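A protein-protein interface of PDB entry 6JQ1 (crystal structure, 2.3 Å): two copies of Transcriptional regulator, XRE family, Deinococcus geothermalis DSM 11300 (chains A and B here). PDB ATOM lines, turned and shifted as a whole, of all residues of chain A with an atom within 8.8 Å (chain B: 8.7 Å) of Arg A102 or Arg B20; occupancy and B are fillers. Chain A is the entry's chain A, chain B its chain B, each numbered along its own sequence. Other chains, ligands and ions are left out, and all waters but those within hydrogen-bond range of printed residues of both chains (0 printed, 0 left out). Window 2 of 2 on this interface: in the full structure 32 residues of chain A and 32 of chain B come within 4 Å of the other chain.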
ATOM      1  N   ALA A  78      27.030 -10.660   4.027  1.00  0.00           N
ATOM      2  CA  ALA A  78      25.753 -11.368   3.975  1.00  0.00           C
ATOM      3  C   ALA A  78      25.673 -12.275   2.751  1.00  0.00           C
ATOM      4  O   ALA A  78      25.095 -13.366   2.813  1.00  0.00           O
ATOM      5  CB  ALA A  78      24.600 -10.363   3.994  1.00  0.00           C
ATOM      6  N   LEU A  79      26.255 -11.848   1.641  1.00  0.00           N
ATOM      7  CA  LEU A  79      26.310 -12.600   0.400  1.00  0.00           C
ATOM      8  C   LEU A  79      27.731 -13.088   0.141  1.00  0.00           C
ATOM      9  O   LEU A  79      28.686 -12.623   0.770  1.00  0.00           O
ATOM     10  CB  LEU A  79      25.854 -11.707  -0.761  1.00  0.00           C
ATOM     11  CG  LEU A  79      24.387 -11.277  -0.747  1.00  0.00           C
ATOM     12  CD1 LEU A  79      24.122 -10.336  -1.903  1.00  0.00           C
ATOM     13  CD2 LEU A  79      23.456 -12.479  -0.805  1.00  0.00           C
ATOM     14  N   PRO A  80      27.902 -14.053  -0.767  1.00  0.00           N
ATOM     15  CA  PRO A  80      29.256 -14.408  -1.210  1.00  0.00           C
ATOM     16  C   PRO A  80      29.948 -13.198  -1.818  1.00  0.00           C
ATOM     17  O   PRO A  80      29.317 -12.347  -2.445  1.00  0.00           O
ATOM     18  CB  PRO A  80      29.008 -15.484  -2.274  1.00  0.00           C
ATOM     19  CG  PRO A  80      27.694 -16.073  -1.906  1.00  0.00           C
ATOM     20  CD  PRO A  80      26.881 -14.942  -1.347  1.00  0.00           C
ATOM     21  N   LEU A  83      29.397 -12.828  -5.616  1.00  0.00           N
ATOM     22  CA  LEU A  83      28.035 -12.383  -5.902  1.00  0.00           C
ATOM     23  C   LEU A  83      27.825 -10.944  -5.454  1.00  0.00           C
ATOM     24  O   LEU A  83      27.145 -10.168  -6.133  1.00  0.00           O
ATOM     25  CB  LEU A  83      27.030 -13.309  -5.216  1.00  0.00           C
ATOM     26  CG  LEU A  83      25.554 -13.039  -5.518  1.00  0.00           C
ATOM     27  CD1 LEU A  83      25.301 -12.996  -7.025  1.00  0.00           C
ATOM     28  CD2 LEU A  83      24.677 -14.086  -4.847  1.00  0.00           C
ATOM     29  N   VAL A  87      26.727  -7.731  -7.782  1.00  0.00           N
ATOM     30  CA  VAL A  87      25.622  -6.821  -7.489  1.00  0.00           C
ATOM     31  C   VAL A  87      26.134  -5.396  -7.311  1.00  0.00           C
ATOM     32  O   VAL A  87      25.484  -4.429  -7.728  1.00  0.00           O
ATOM     33  CB  VAL A  87      24.826  -7.313  -6.263  1.00  0.00           C
ATOM     34  CG1 VAL A  87      23.647  -6.386  -5.976  1.00  0.00           C
ATOM     35  CG2 VAL A  87      24.339  -8.743  -6.473  1.00  0.00           C
ATOM     36  N   ILE A  96      20.112  -7.911 -13.244  1.00  0.00           N
ATOM     37  CA  ILE A  96      19.844  -9.046 -12.371  1.00  0.00           C
ATOM     38  C   ILE A  96      18.805  -8.654 -11.333  1.00  0.00           C
ATOM     39  O   ILE A  96      18.921  -7.617 -10.666  1.00  0.00           O
ATOM     40  CB  ILE A  96      21.137  -9.560 -11.725  1.00  0.00           C
ATOM     41  CG1 ILE A  96      22.076 -10.134 -12.787  1.00  0.00           C
ATOM     42  CG2 ILE A  96      20.825 -10.619 -10.672  1.00  0.00           C
ATOM     43  CD1 ILE A  96      23.295 -10.802 -12.204  1.00  0.00           C
ATOM     44  N   THR A  97      17.707  -9.412 -11.296  1.00  0.00           N
ATOM     45  CA  THR A  97      16.621  -9.105 -10.332  1.00  0.00           C
ATOM     46  C   THR A  97      17.011  -9.574  -8.933  1.00  0.00           C
ATOM     47  O   THR A  97      17.857 -10.467  -8.805  1.00  0.00           O
ATOM     48  CB  THR A  97      15.247  -9.649 -10.737  1.00  0.00           C
ATOM     49  OG1 THR A  97      15.246 -11.063 -10.545  1.00  0.00           O
ATOM     50  CG2 THR A  97      14.846  -9.284 -12.146  1.00  0.00           C
ATOM     51  N   PRO A  98      16.443  -8.955  -7.887  1.00  0.00           N
ATOM     52  CA  PRO A  98      16.746  -9.317  -6.490  1.00  0.00           C
ATOM     53  C   PRO A  98      16.414 -10.760  -6.156  1.00  0.00           C
ATOM     54  O   PRO A  98      17.180 -11.421  -5.443  1.00  0.00           O
ATOM     55  CB  PRO A  98      15.900  -8.327  -5.678  1.00  0.00           C
ATOM     56  CG  PRO A  98      15.669  -7.178  -6.609  1.00  0.00           C
ATOM     57  CD  PRO A  98      15.570  -7.772  -7.978  1.00  0.00           C
ATOM     58  N   ASP A  99      15.280 -11.264  -6.650  1.00  0.00           N
ATOM     59  CA  ASP A  99      14.960 -12.680  -6.497  1.00  0.00           C
ATOM     60  C   ASP A  99      16.057 -13.554  -7.094  1.00  0.00           C
ATOM     61  O   ASP A  99      16.417 -14.591  -6.521  1.00  0.00           O
ATOM     62  CB  ASP A  99      13.624 -12.989  -7.166  1.00  0.00           C
ATOM     63  CG  ASP A  99      12.477 -12.197  -6.578  1.00  0.00           C
ATOM     64  OD1 ASP A  99      12.168 -12.391  -5.384  1.00  0.00           O
ATOM     65  OD2 ASP A  99      11.888 -11.372  -7.309  1.00  0.00           O
ATOM     66  N   TRP A 100      16.597 -13.154  -8.249  1.00  0.00           N
ATOM     67  CA  TRP A 100      17.704 -13.899  -8.841  1.00  0.00           C
ATOM     68  C   TRP A 100      18.934 -13.869  -7.944  1.00  0.00           C
ATOM     69  O   TRP A 100      19.651 -14.871  -7.834  1.00  0.00           O
ATOM     70  CB  TRP A 100      18.029 -13.365 -10.237  1.00  0.00           C
ATOM     71  CG  TRP A 100      17.406 -14.172 -11.326  1.00  0.00           C
ATOM     72  CD1 TRP A 100      16.491 -13.747 -12.241  1.00  0.00           C
ATOM     73  CD2 TRP A 100      17.636 -15.560 -11.605  1.00  0.00           C
ATOM     74  NE1 TRP A 100      16.143 -14.777 -13.079  1.00  0.00           N
ATOM     75  CE2 TRP A 100      16.831 -15.901 -12.710  1.00  0.00           C
ATOM     76  CE3 TRP A 100      18.447 -16.546 -11.032  1.00  0.00           C
ATOM     77  CZ2 TRP A 100      16.813 -17.181 -13.254  1.00  0.00           C
ATOM     78  CZ3 TRP A 100      18.427 -17.819 -11.574  1.00  0.00           C
ATOM     79  CH2 TRP A 100      17.615 -18.125 -12.675  1.00  0.00           C
ATOM     80  N   VAL A 101      19.198 -12.727  -7.299  1.00  0.00           N
ATOM     81  CA  VAL A 101      20.301 -12.645  -6.342  1.00  0.00           C
ATOM     82  C   VAL A 101      20.092 -13.641  -5.207  1.00  0.00           C
ATOM     83  O   VAL A 101      21.017 -14.361  -4.814  1.00  0.00           O
ATOM     84  CB  VAL A 101      20.463 -11.202  -5.824  1.00  0.00           C
ATOM     85  CG1 VAL A 101      21.726 -11.077  -4.968  1.00  0.00           C
ATOM     86  CG2 VAL A 101      20.479 -10.208  -6.982  1.00  0.00           C
ATOM     87  N   ARG A 102      18.865 -13.718  -4.682  1.00  0.00           N
ATOM     88  CA  ARG A 102      18.574 -14.647  -3.594  1.00  0.00           C
ATOM     89  C   ARG A 102      18.756 -16.095  -4.039  1.00  0.00           C
ATOM     90  O   ARG A 102      19.343 -16.908  -3.315  1.00  0.00           O
ATOM     91  CB  ARG A 102      17.154 -14.419  -3.091  1.00  0.00           C
ATOM     92  CG  ARG A 102      16.948 -14.797  -1.646  1.00  0.00           C
ATOM     93  CD  ARG A 102      15.477 -14.839  -1.318  1.00  0.00           C
ATOM     94  NE  ARG A 102      14.732 -13.751  -1.947  1.00  0.00           N
ATOM     95  CZ  ARG A 102      14.668 -12.513  -1.470  1.00  0.00           C
ATOM     96  NH1 ARG A 102      15.323 -12.191  -0.358  1.00  0.00           N
ATOM     97  NH2 ARG A 102      13.953 -11.597  -2.105  1.00  0.00           N
ATOM     98  N   THR A 103      18.221 -16.441  -5.215  1.00  0.00           N
ATOM     99  CA  THR A 103      18.424 -17.773  -5.785  1.00  0.00           C
ATOM    100  C   THR A 103      19.910 -18.101  -5.880  1.00  0.00           C
ATOM    101  O   THR A 103      20.353 -19.177  -5.451  1.00  0.00           O
ATOM    102  CB  THR A 103      17.781 -17.836  -7.175  1.00  0.00           C
ATOM    103  OG1 THR A 103      16.353 -17.773  -7.062  1.00  0.00           O
ATOM    104  CG2 THR A 103      18.192 -19.112  -7.924  1.00  0.00           C
ATOM    105  N   LEU A 104      20.693 -17.174  -6.441  1.00  0.00           N
ATOM    106  CA  LEU A 104      22.127 -17.386  -6.614  1.00  0.00           C
ATOM    107  C   LEU A 104      22.865 -17.514  -5.287  1.00  0.00           C
ATOM    108  O   LEU A 104      23.839 -18.270  -5.196  1.00  0.00           O
ATOM    109  CB  LEU A 104      22.716 -16.235  -7.433  1.00  0.00           C
ATOM    110  CG  LEU A 104      22.392 -16.262  -8.924  1.00  0.00           C
ATOM    111  CD1 LEU A 104      22.473 -14.864  -9.516  1.00  0.00           C
ATOM    112  CD2 LEU A 104      23.326 -17.219  -9.655  1.00  0.00           C
ATOM    113  N   SER A 105      22.424 -16.789  -4.254  1.00  0.00           N
ATOM    114  CA  SER A 105      23.142 -16.797  -2.982  1.00  0.00           C
ATOM    115  C   SER A 105      23.130 -18.170  -2.321  1.00  0.00           C
ATOM    116  O   SER A 105      24.065 -18.510  -1.589  1.00  0.00           O
ATOM    117  CB  SER A 105      22.575 -15.735  -2.042  1.00  0.00           C
ATOM    118  OG  SER A 105      21.187 -15.924  -1.837  1.00  0.00           O
ATOM    119  N   ARG A 106      22.090 -18.974  -2.565  1.00  0.00           N
ATOM    120  CA  ARG A 106      22.025 -20.293  -1.944  1.00  0.00           C
ATOM    121  C   ARG A 106      23.083 -21.241  -2.503  1.00  0.00           C
ATOM    122  O   ARG A 106      23.500 -22.177  -1.814  1.00  0.00           O
ATOM    123  CB  ARG A 106      20.626 -20.888  -2.094  1.00  0.00           C
ATOM    124  CG  ARG A 106      19.521 -20.031  -1.506  1.00  0.00           C
ATOM    125  CD  ARG A 106      18.221 -20.805  -1.395  1.00  0.00           C
ATOM    126  NE  ARG A 106      17.135 -19.961  -0.912  1.00  0.00           N
ATOM    127  CZ  ARG A 106      16.210 -19.419  -1.695  1.00  0.00           C
ATOM    128  NH1 ARG A 106      16.237 -19.645  -3.001  1.00  0.00           N
ATOM    129  NH2 ARG A 106      15.255 -18.659  -1.176  1.00  0.00           N
ATOM    130  N   ILE A 107      23.535 -21.012  -3.737  1.00  0.00           N
ATOM    131  CA  ILE A 107      24.534 -21.878  -4.359  1.00  0.00           C
ATOM    132  C   ILE A 107      25.874 -21.724  -3.653  1.00  0.00           C
ATOM    133  O   ILE A 107      26.425 -20.618  -3.579  1.00  0.00           O
ATOM    134  CB  ILE A 107      24.671 -21.541  -5.849  1.00  0.00           C
ATOM    135  CG1 ILE A 107      23.342 -21.742  -6.577  1.00  0.00           C
ATOM    136  CG2 ILE A 107      25.787 -22.365  -6.486  1.00  0.00           C
ATOM    137  CD1 ILE A 107      23.309 -21.120  -7.950  1.00  0.00           C
ATOM    138  N   TRP A 120      30.072 -15.651 -11.346  1.00  0.00           N
ATOM    139  CA  TRP A 120      28.683 -15.551 -10.902  1.00  0.00           C
ATOM    140  C   TRP A 120      27.765 -15.091 -12.027  1.00  0.00           C
ATOM    141  O   TRP A 120      26.637 -15.583 -12.151  1.00  0.00           O
ATOM    142  CB  TRP A 120      28.569 -14.614  -9.695  1.00  0.00           C
ATOM    143  CG  TRP A 120      28.999 -15.259  -8.414  1.00  0.00           C
ATOM    144  CD1 TRP A 120      30.199 -15.109  -7.783  1.00  0.00           C
ATOM    145  CD2 TRP A 120      28.241 -16.185  -7.620  1.00  0.00           C
ATOM    146  NE1 TRP A 120      30.233 -15.873  -6.642  1.00  0.00           N
ATOM    147  CE2 TRP A 120      29.045 -16.544  -6.519  1.00  0.00           C
ATOM    148  CE3 TRP A 120      26.963 -16.741  -7.732  1.00  0.00           C
ATOM    149  CZ2 TRP A 120      28.613 -17.433  -5.536  1.00  0.00           C
ATOM    150  CZ3 TRP A 120      26.533 -17.625  -6.750  1.00  0.00           C
ATOM    151  CH2 TRP A 120      27.357 -17.961  -5.669  1.00  0.00           C
ATOM    152  N   ARG B  14      19.962  -3.342   0.805  1.00  0.00           N
ATOM    153  CA  ARG B  14      19.288  -4.585   1.175  1.00  0.00           C
ATOM    154  C   ARG B  14      18.277  -5.009   0.116  1.00  0.00           C
ATOM    155  O   ARG B  14      18.191  -6.195  -0.227  1.00  0.00           O
ATOM    156  CB  ARG B  14      18.601  -4.424   2.535  1.00  0.00           C
ATOM    157  CG  ARG B  14      18.007  -5.714   3.078  1.00  0.00           C
ATOM    158  CD  ARG B  14      17.394  -5.526   4.459  1.00  0.00           C
ATOM    159  NE  ARG B  14      16.261  -4.606   4.442  1.00  0.00           N
ATOM    160  CZ  ARG B  14      15.008  -4.971   4.189  1.00  0.00           C
ATOM    161  NH1 ARG B  14      14.728  -6.240   3.926  1.00  0.00           N
ATOM    162  NH2 ARG B  14      14.032  -4.072   4.197  1.00  0.00           N
ATOM    163  N   SER B  15      17.505  -4.051  -0.414  1.00  0.00           N
ATOM    164  CA  SER B  15      16.446  -4.376  -1.367  1.00  0.00           C
ATOM    165  C   SER B  15      16.998  -4.938  -2.673  1.00  0.00           C
ATOM    166  O   SER B  15      16.494  -5.948  -3.175  1.00  0.00           O
ATOM    167  CB  SER B  15      15.583  -3.142  -1.639  1.00  0.00           C
ATOM    168  OG  SER B  15      14.876  -3.278  -2.859  1.00  0.00           O
ATOM    169  N   GLU B  16      18.028  -4.302  -3.243  1.00  0.00           N
ATOM    170  CA  GLU B  16      18.562  -4.780  -4.518  1.00  0.00           C
ATOM    171  C   GLU B  16      19.221  -6.149  -4.388  1.00  0.00           C
ATOM    172  O   GLU B  16      19.290  -6.895  -5.368  1.00  0.00           O
ATOM    173  CB  GLU B  16      19.527  -3.759  -5.125  1.00  0.00           C
ATOM    174  CG  GLU B  16      20.846  -3.639  -4.393  1.00  0.00           C
ATOM    175  CD  GLU B  16      21.708  -2.521  -4.940  1.00  0.00           C
ATOM    176  OE1 GLU B  16      21.319  -1.923  -5.965  1.00  0.00           O
ATOM    177  OE2 GLU B  16      22.770  -2.240  -4.345  1.00  0.00           O
ATOM    178  N   ARG B  17      19.705  -6.499  -3.198  1.00  0.00           N
ATOM    179  CA  ARG B  17      20.290  -7.812  -2.953  1.00  0.00           C
ATOM    180  C   ARG B  17      19.245  -8.846  -2.558  1.00  0.00           C
ATOM    181  O   ARG B  17      19.599 -10.012  -2.344  1.00  0.00           O
ATOM    182  CB  ARG B  17      21.367  -7.725  -1.872  1.00  0.00           C
ATOM    183  CG  ARG B  17      22.640  -7.070  -2.356  1.00  0.00           C
ATOM    184  CD  ARG B  17      23.429  -6.466  -1.218  1.00  0.00           C
ATOM    185  NE  ARG B  17      24.683  -5.910  -1.706  1.00  0.00           N
ATOM    186  CZ  ARG B  17      24.778  -4.770  -2.381  1.00  0.00           C
ATOM    187  NH1 ARG B  17      23.689  -4.065  -2.652  1.00  0.00           N
ATOM    188  NH2 ARG B  17      25.965  -4.337  -2.788  1.00  0.00           N
ATOM    189  N   GLY B  18      17.978  -8.444  -2.479  1.00  0.00           N
ATOM    190  CA  GLY B  18      16.922  -9.307  -2.011  1.00  0.00           C
ATOM    191  C   GLY B  18      17.308 -10.021  -0.731  1.00  0.00           C
ATOM    192  O   GLY B  18      17.339 -11.258  -0.689  1.00  0.00           O
ATOM    193  N   LEU B  19      17.651  -9.261   0.306  1.00  0.00           N
ATOM    194  CA  LEU B  19      17.956  -9.807   1.619  1.00  0.00           C
ATOM    195  C   LEU B  19      16.843  -9.437   2.587  1.00  0.00           C
ATOM    196  O   LEU B  19      16.352  -8.303   2.586  1.00  0.00           O
ATOM    197  CB  LEU B  19      19.300  -9.284   2.142  1.00  0.00           C
ATOM    198  CG  LEU B  19      20.521  -9.905   1.448  1.00  0.00           C
ATOM    199  CD1 LEU B  19      21.794  -9.097   1.699  1.00  0.00           C
ATOM    200  CD2 LEU B  19      20.710 -11.377   1.846  1.00  0.00           C
ATOM    201  N   ARG B  20      16.430 -10.404   3.394  1.00  0.00           N
ATOM    202  CA  ARG B  20      15.472 -10.120   4.447  1.00  0.00           C
ATOM    203  C   ARG B  20      16.155  -9.392   5.603  1.00  0.00           C
ATOM    204  O   ARG B  20      17.381  -9.431   5.758  1.00  0.00           O
ATOM    205  CB  ARG B  20      14.779 -11.407   4.896  1.00  0.00           C
ATOM    206  CG  ARG B  20      13.702 -11.839   3.916  1.00  0.00           C
ATOM    207  CD  ARG B  20      13.381 -13.315   4.003  1.00  0.00           C
ATOM    208  NE  ARG B  20      12.403 -13.686   2.985  1.00  0.00           N
ATOM    209  CZ  ARG B  20      12.717 -14.071   1.752  1.00  0.00           C
ATOM    210  NH1 ARG B  20      11.759 -14.380   0.888  1.00  0.00           N
ATOM    211  NH2 ARG B  20      13.987 -14.152   1.385  1.00  0.00           N
ATOM    212  N   LEU B  21      15.345  -8.688   6.399  1.00  0.00           N
ATOM    213  CA  LEU B  21      15.899  -7.900   7.499  1.00  0.00           C
ATOM    214  C   LEU B  21      16.686  -8.771   8.470  1.00  0.00           C
ATOM    215  O   LEU B  21      17.766  -8.378   8.927  1.00  0.00           O
ATOM    216  CB  LEU B  21      14.790  -7.142   8.230  1.00  0.00           C
ATOM    217  CG  LEU B  21      14.297  -5.856   7.563  1.00  0.00           C
ATOM    218  CD1 LEU B  21      12.985  -5.401   8.188  1.00  0.00           C
ATOM    219  CD2 LEU B  21      15.355  -4.761   7.655  1.00  0.00           C
ATOM    220  N   LYS B  22      16.165  -9.964   8.786  1.00  0.00           N
ATOM    221  CA  LYS B  22      16.852 -10.845   9.727  1.00  0.00           C
ATOM    222  C   LYS B  22      18.227 -11.253   9.212  1.00  0.00           C
ATOM    223  O   LYS B  22      19.199 -11.263   9.975  1.00  0.00           O
ATOM    224  CB  LYS B  22      15.989 -12.067  10.049  1.00  0.00           C
ATOM    225  CG  LYS B  22      15.501 -12.851   8.845  1.00  0.00           C
ATOM    226  CD  LYS B  22      14.617 -14.003   9.291  1.00  0.00           C
ATOM    227  CE  LYS B  22      13.939 -14.685   8.116  1.00  0.00           C
ATOM    228  NZ  LYS B  22      14.941 -15.237   7.167  1.00  0.00           N
ATOM    229  N   ASP B  23      18.333 -11.573   7.916  1.00  0.00           N
ATOM    230  CA  ASP B  23      19.624 -11.934   7.332  1.00  0.00           C
ATOM    231  C   ASP B  23      20.661 -10.848   7.587  1.00  0.00           C
ATOM    232  O   ASP B  23      21.745 -11.121   8.117  1.00  0.00           O
ATOM    233  CB  ASP B  23      19.474 -12.156   5.825  1.00  0.00           C
ATOM    234  CG  ASP B  23      18.331 -13.085   5.481  1.00  0.00           C
ATOM    235  OD1 ASP B  23      18.105 -14.060   6.229  1.00  0.00           O
ATOM    236  OD2 ASP B  23      17.656 -12.835   4.459  1.00  0.00           O
ATOM    237  N   VAL B  24      20.343  -9.606   7.207  1.00  0.00           N
ATOM    238  CA  VAL B  24      21.260  -8.490   7.432  1.00  0.00           C
ATOM    239  C   VAL B  24      21.510  -8.294   8.924  1.00  0.00           C
ATOM    240  O   VAL B  24      22.653  -8.085   9.350  1.00  0.00           O
ATOM    241  CB  VAL B  24      20.733  -7.207   6.757  1.00  0.00           C
ATOM    242  CG1 VAL B  24      21.701  -6.037   6.968  1.00  0.00           C
ATOM    243  CG2 VAL B  24      20.477  -7.442   5.271  1.00  0.00           C
ATOM    244  N   ALA B  25      20.453  -8.368   9.740  1.00  0.00           N
ATOM    245  CA  ALA B  25      20.600  -8.122  11.174  1.00  0.00           C
ATOM    246  C   ALA B  25      21.498  -9.165  11.824  1.00  0.00           C
ATOM    247  O   ALA B  25      22.429  -8.826  12.566  1.00  0.00           O
ATOM    248  CB  ALA B  25      19.228  -8.113  11.846  1.00  0.00           C
ATOM    249  N   GLU B  26      21.222 -10.446  11.570  1.00  0.00           N
ATOM    250  CA  GLU B  26      22.056 -11.502  12.132  1.00  0.00           C
ATOM    251  C   GLU B  26      23.502 -11.358  11.675  1.00  0.00           C
ATOM    252  O   GLU B  26      24.431 -11.558  12.464  1.00  0.00           O
ATOM    253  CB  GLU B  26      21.494 -12.873  11.750  1.00  0.00           C
ATOM    254  CG  GLU B  26      20.066 -13.115  12.225  1.00  0.00           C
ATOM    255  CD  GLU B  26      19.548 -14.492  11.852  1.00  0.00           C
ATOM    256  OE1 GLU B  26      20.346 -15.453  11.866  1.00  0.00           O
ATOM    257  OE2 GLU B  26      18.343 -14.613  11.539  1.00  0.00           O
ATOM    258  N   THR B  27      23.710 -10.999  10.403  1.00  0.00           N
ATOM    259  CA  THR B  27      25.065 -10.797   9.896  1.00  0.00           C
ATOM    260  C   THR B  27      25.737  -9.629  10.601  1.00  0.00           C
ATOM    261  O   THR B  27      26.902  -9.722  11.005  1.00  0.00           O
ATOM    262  CB  THR B  27      25.025 -10.547   8.387  1.00  0.00           C
ATOM    263  OG1 THR B  27      24.047 -11.402   7.782  1.00  0.00           O
ATOM    264  CG2 THR B  27      26.388 -10.821   7.755  1.00  0.00           C
ATOM    265  N   VAL B  32      16.620  -6.627  14.392  1.00  0.00           N
ATOM    266  CA  VAL B  32      15.736  -6.166  13.321  1.00  0.00           C
ATOM    267  C   VAL B  32      15.097  -4.810  13.620  1.00  0.00           C
ATOM    268  O   VAL B  32      15.118  -3.936  12.747  1.00  0.00           O
ATOM    269  CB  VAL B  32      14.726  -7.260  12.945  1.00  0.00           C
ATOM    270  CG1 VAL B  32      13.661  -6.717  11.998  1.00  0.00           C
ATOM    271  CG2 VAL B  32      15.442  -8.450  12.316  1.00  0.00           C
ATOM    272  N   LEU B  35      17.771  -2.129  12.976  1.00  0.00           N
ATOM    273  CA  LEU B  35      18.004  -2.012  11.541  1.00  0.00           C
ATOM    274  C   LEU B  35      16.832  -1.316  10.866  1.00  0.00           C
ATOM    275  O   LEU B  35      17.021  -0.423  10.032  1.00  0.00           O
ATOM    276  CB  LEU B  35      18.208  -3.393  10.927  1.00  0.00           C
ATOM    277  CG  LEU B  35      18.507  -3.431   9.425  1.00  0.00           C
ATOM    278  CD1 LEU B  35      19.652  -2.489   9.065  1.00  0.00           C
ATOM    279  CD2 LEU B  35      18.811  -4.857   8.976  1.00  0.00           C
ATOM    280  N   GLU B  39      16.893   1.968   8.595  1.00  0.00           N
ATOM    281  CA  GLU B  39      16.379   2.026   7.231  1.00  0.00           C
ATOM    282  C   GLU B  39      15.286   3.075   7.066  1.00  0.00           C
ATOM    283  O   GLU B  39      15.181   3.686   5.997  1.00  0.00           O
ATOM    284  CB  GLU B  39      15.871   0.651   6.805  1.00  0.00           C
ATOM    285  CG  GLU B  39      16.962  -0.273   6.318  1.00  0.00           C
ATOM    286  CD  GLU B  39      16.408  -1.556   5.751  1.00  0.00           C
ATOM    287  OE1 GLU B  39      15.173  -1.634   5.577  1.00  0.00           O
ATOM    288  OE2 GLU B  39      17.206  -2.479   5.490  1.00  0.00           O
ATOM    289  N   TYR B  57      27.221  -5.712   3.535  1.00  0.00           N
ATOM    290  CA  TYR B  57      26.998  -5.585   2.100  1.00  0.00           C
ATOM    291  C   TYR B  57      28.277  -5.741   1.282  1.00  0.00           C
ATOM    292  O   TYR B  57      28.250  -5.533   0.064  1.00  0.00           O
ATOM    293  CB  TYR B  57      26.291  -4.264   1.778  1.00  0.00           C
ATOM    294  CG  TYR B  57      24.932  -4.144   2.436  1.00  0.00           C
ATOM    295  CD1 TYR B  57      23.904  -5.016   2.105  1.00  0.00           C
ATOM    296  CD2 TYR B  57      24.678  -3.168   3.391  1.00  0.00           C
ATOM    297  CE1 TYR B  57      22.660  -4.920   2.709  1.00  0.00           C
ATOM    298  CE2 TYR B  57      23.438  -3.063   3.998  1.00  0.00           C
ATOM    299  CZ  TYR B  57      22.432  -3.943   3.655  1.00  0.00           C
ATOM    300  OH  TYR B  57      21.200  -3.838   4.260  1.00  0.00           O
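The guanidinium group of Arg A102 lies close to the backbone carbonyl oxygen of Gly B18 (2.2 Å).
The guanidinium group (NH1) of Arg A102 sits close to the guanidinium group (NH2) of Arg B20 (2.9 Å).
OD1 of Asp A99 is in salt-bridge range of NH2 of Arg A102, at 3.8 Å.
O of Val A101 lies within hydrogen-bond range of OG of Ser A105.
The side-chain hydroxyl of Ser A105 lies within hydrogen-bond range of the backbone carbonyl oxygen of Arg A102, at 2.6 Å.
The backbone carbonyl oxygen (O) of Leu B19 is in hydrogen-bond range of the guanidinium group (NH1) of Arg B14.
NH1 of Arg B17 lies within salt-bridge range of OE2 of Glu B16 (2.7 Å).
The backbone NH (N) of Arg B20 sits at hydrogen-bond distance from the side-chain carboxylate (OD2) of Asp B23, at 2.9 Å.
CB of Ala A78 touches CD1 of Leu B19, 3.8 Å away.
Ala A78 touches Thr B27 (N to CG2, 3.8 Å).
CG of Arg B17 touches CD1 of Leu A79 (3.6 Å).
Arg B17 touches Val A87 (CG to CG1, 3.8 Å).
Pro A98 touches Ser B15 (CB to O, 3.5 Å).
Glu B16 touches Pro A98 (O to CA, 3.7 Å).
Pro A98 touches Gly B18 (CB to N, 3.8 Å).
O of Glu B16 touches CG2 of Val A101, 3.9 Å away.
Arg B17 touches Val A101 (O to CG1, 3.5 Å).
NH1 of Arg A102 touches N of Leu B19, at 3.8 Å.
Of the printed residues of chain B, Ala A78 touches Leu B19 and Thr B27.
Val A101 touches just these residues of chain B: Glu B16 and Arg B17.
Of chain B, only Gly B18, Leu B19 and Arg B20 come within 4 Å of Arg A102.
Of the printed residues of chain A, Glu B16 touches Pro A98 and Val A101.
Printed residues of chain A within 4 Å of Arg B17: Leu A79, Val A87 and Val A101.
Of chain A, only Arg A102 (2.9 Å) comes within 4 Å of Arg B20.
Ala B25 touches none of the printed residues of chain A.
Printed residues of chain A within 4 Å of Thr B27: Ala A78.
Val B32 touches none of the printed residues of chain A.
The nearest residue of chain B that does not touch Arg A102 is Arg B17 (4.4 Å).
The nearest residue of chain A that does not touch Arg B20 is Arg A106 (5.3 Å).
The nearest printed residue of chain A that does not touch Gly B18 is Val A101 (5.0 Å).
Printed residues of chain A that touch a printed residue of chain B: Ala A78, Leu A79, Val A87, Pro A98, Val A101 and Arg A102.
Printed residues of chain B that touch a printed residue of chain A: Ser B15, Glu B16, Arg B17, Gly B18, Leu B19, Arg B20 and Thr B27.
Hydrophobic or aromatic side chains of chain B that line the printed part of chain A: Leu B19.
Among the printed residues, no Asp or Glu carboxylate lies within 4 Å of a Lys or Arg side-chain nitrogen of the other chain.
No position is printed for both chains.
Of the 13 pairs that touch across the chains among the printed residues, none has its exchanged pair printed and touching as well.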
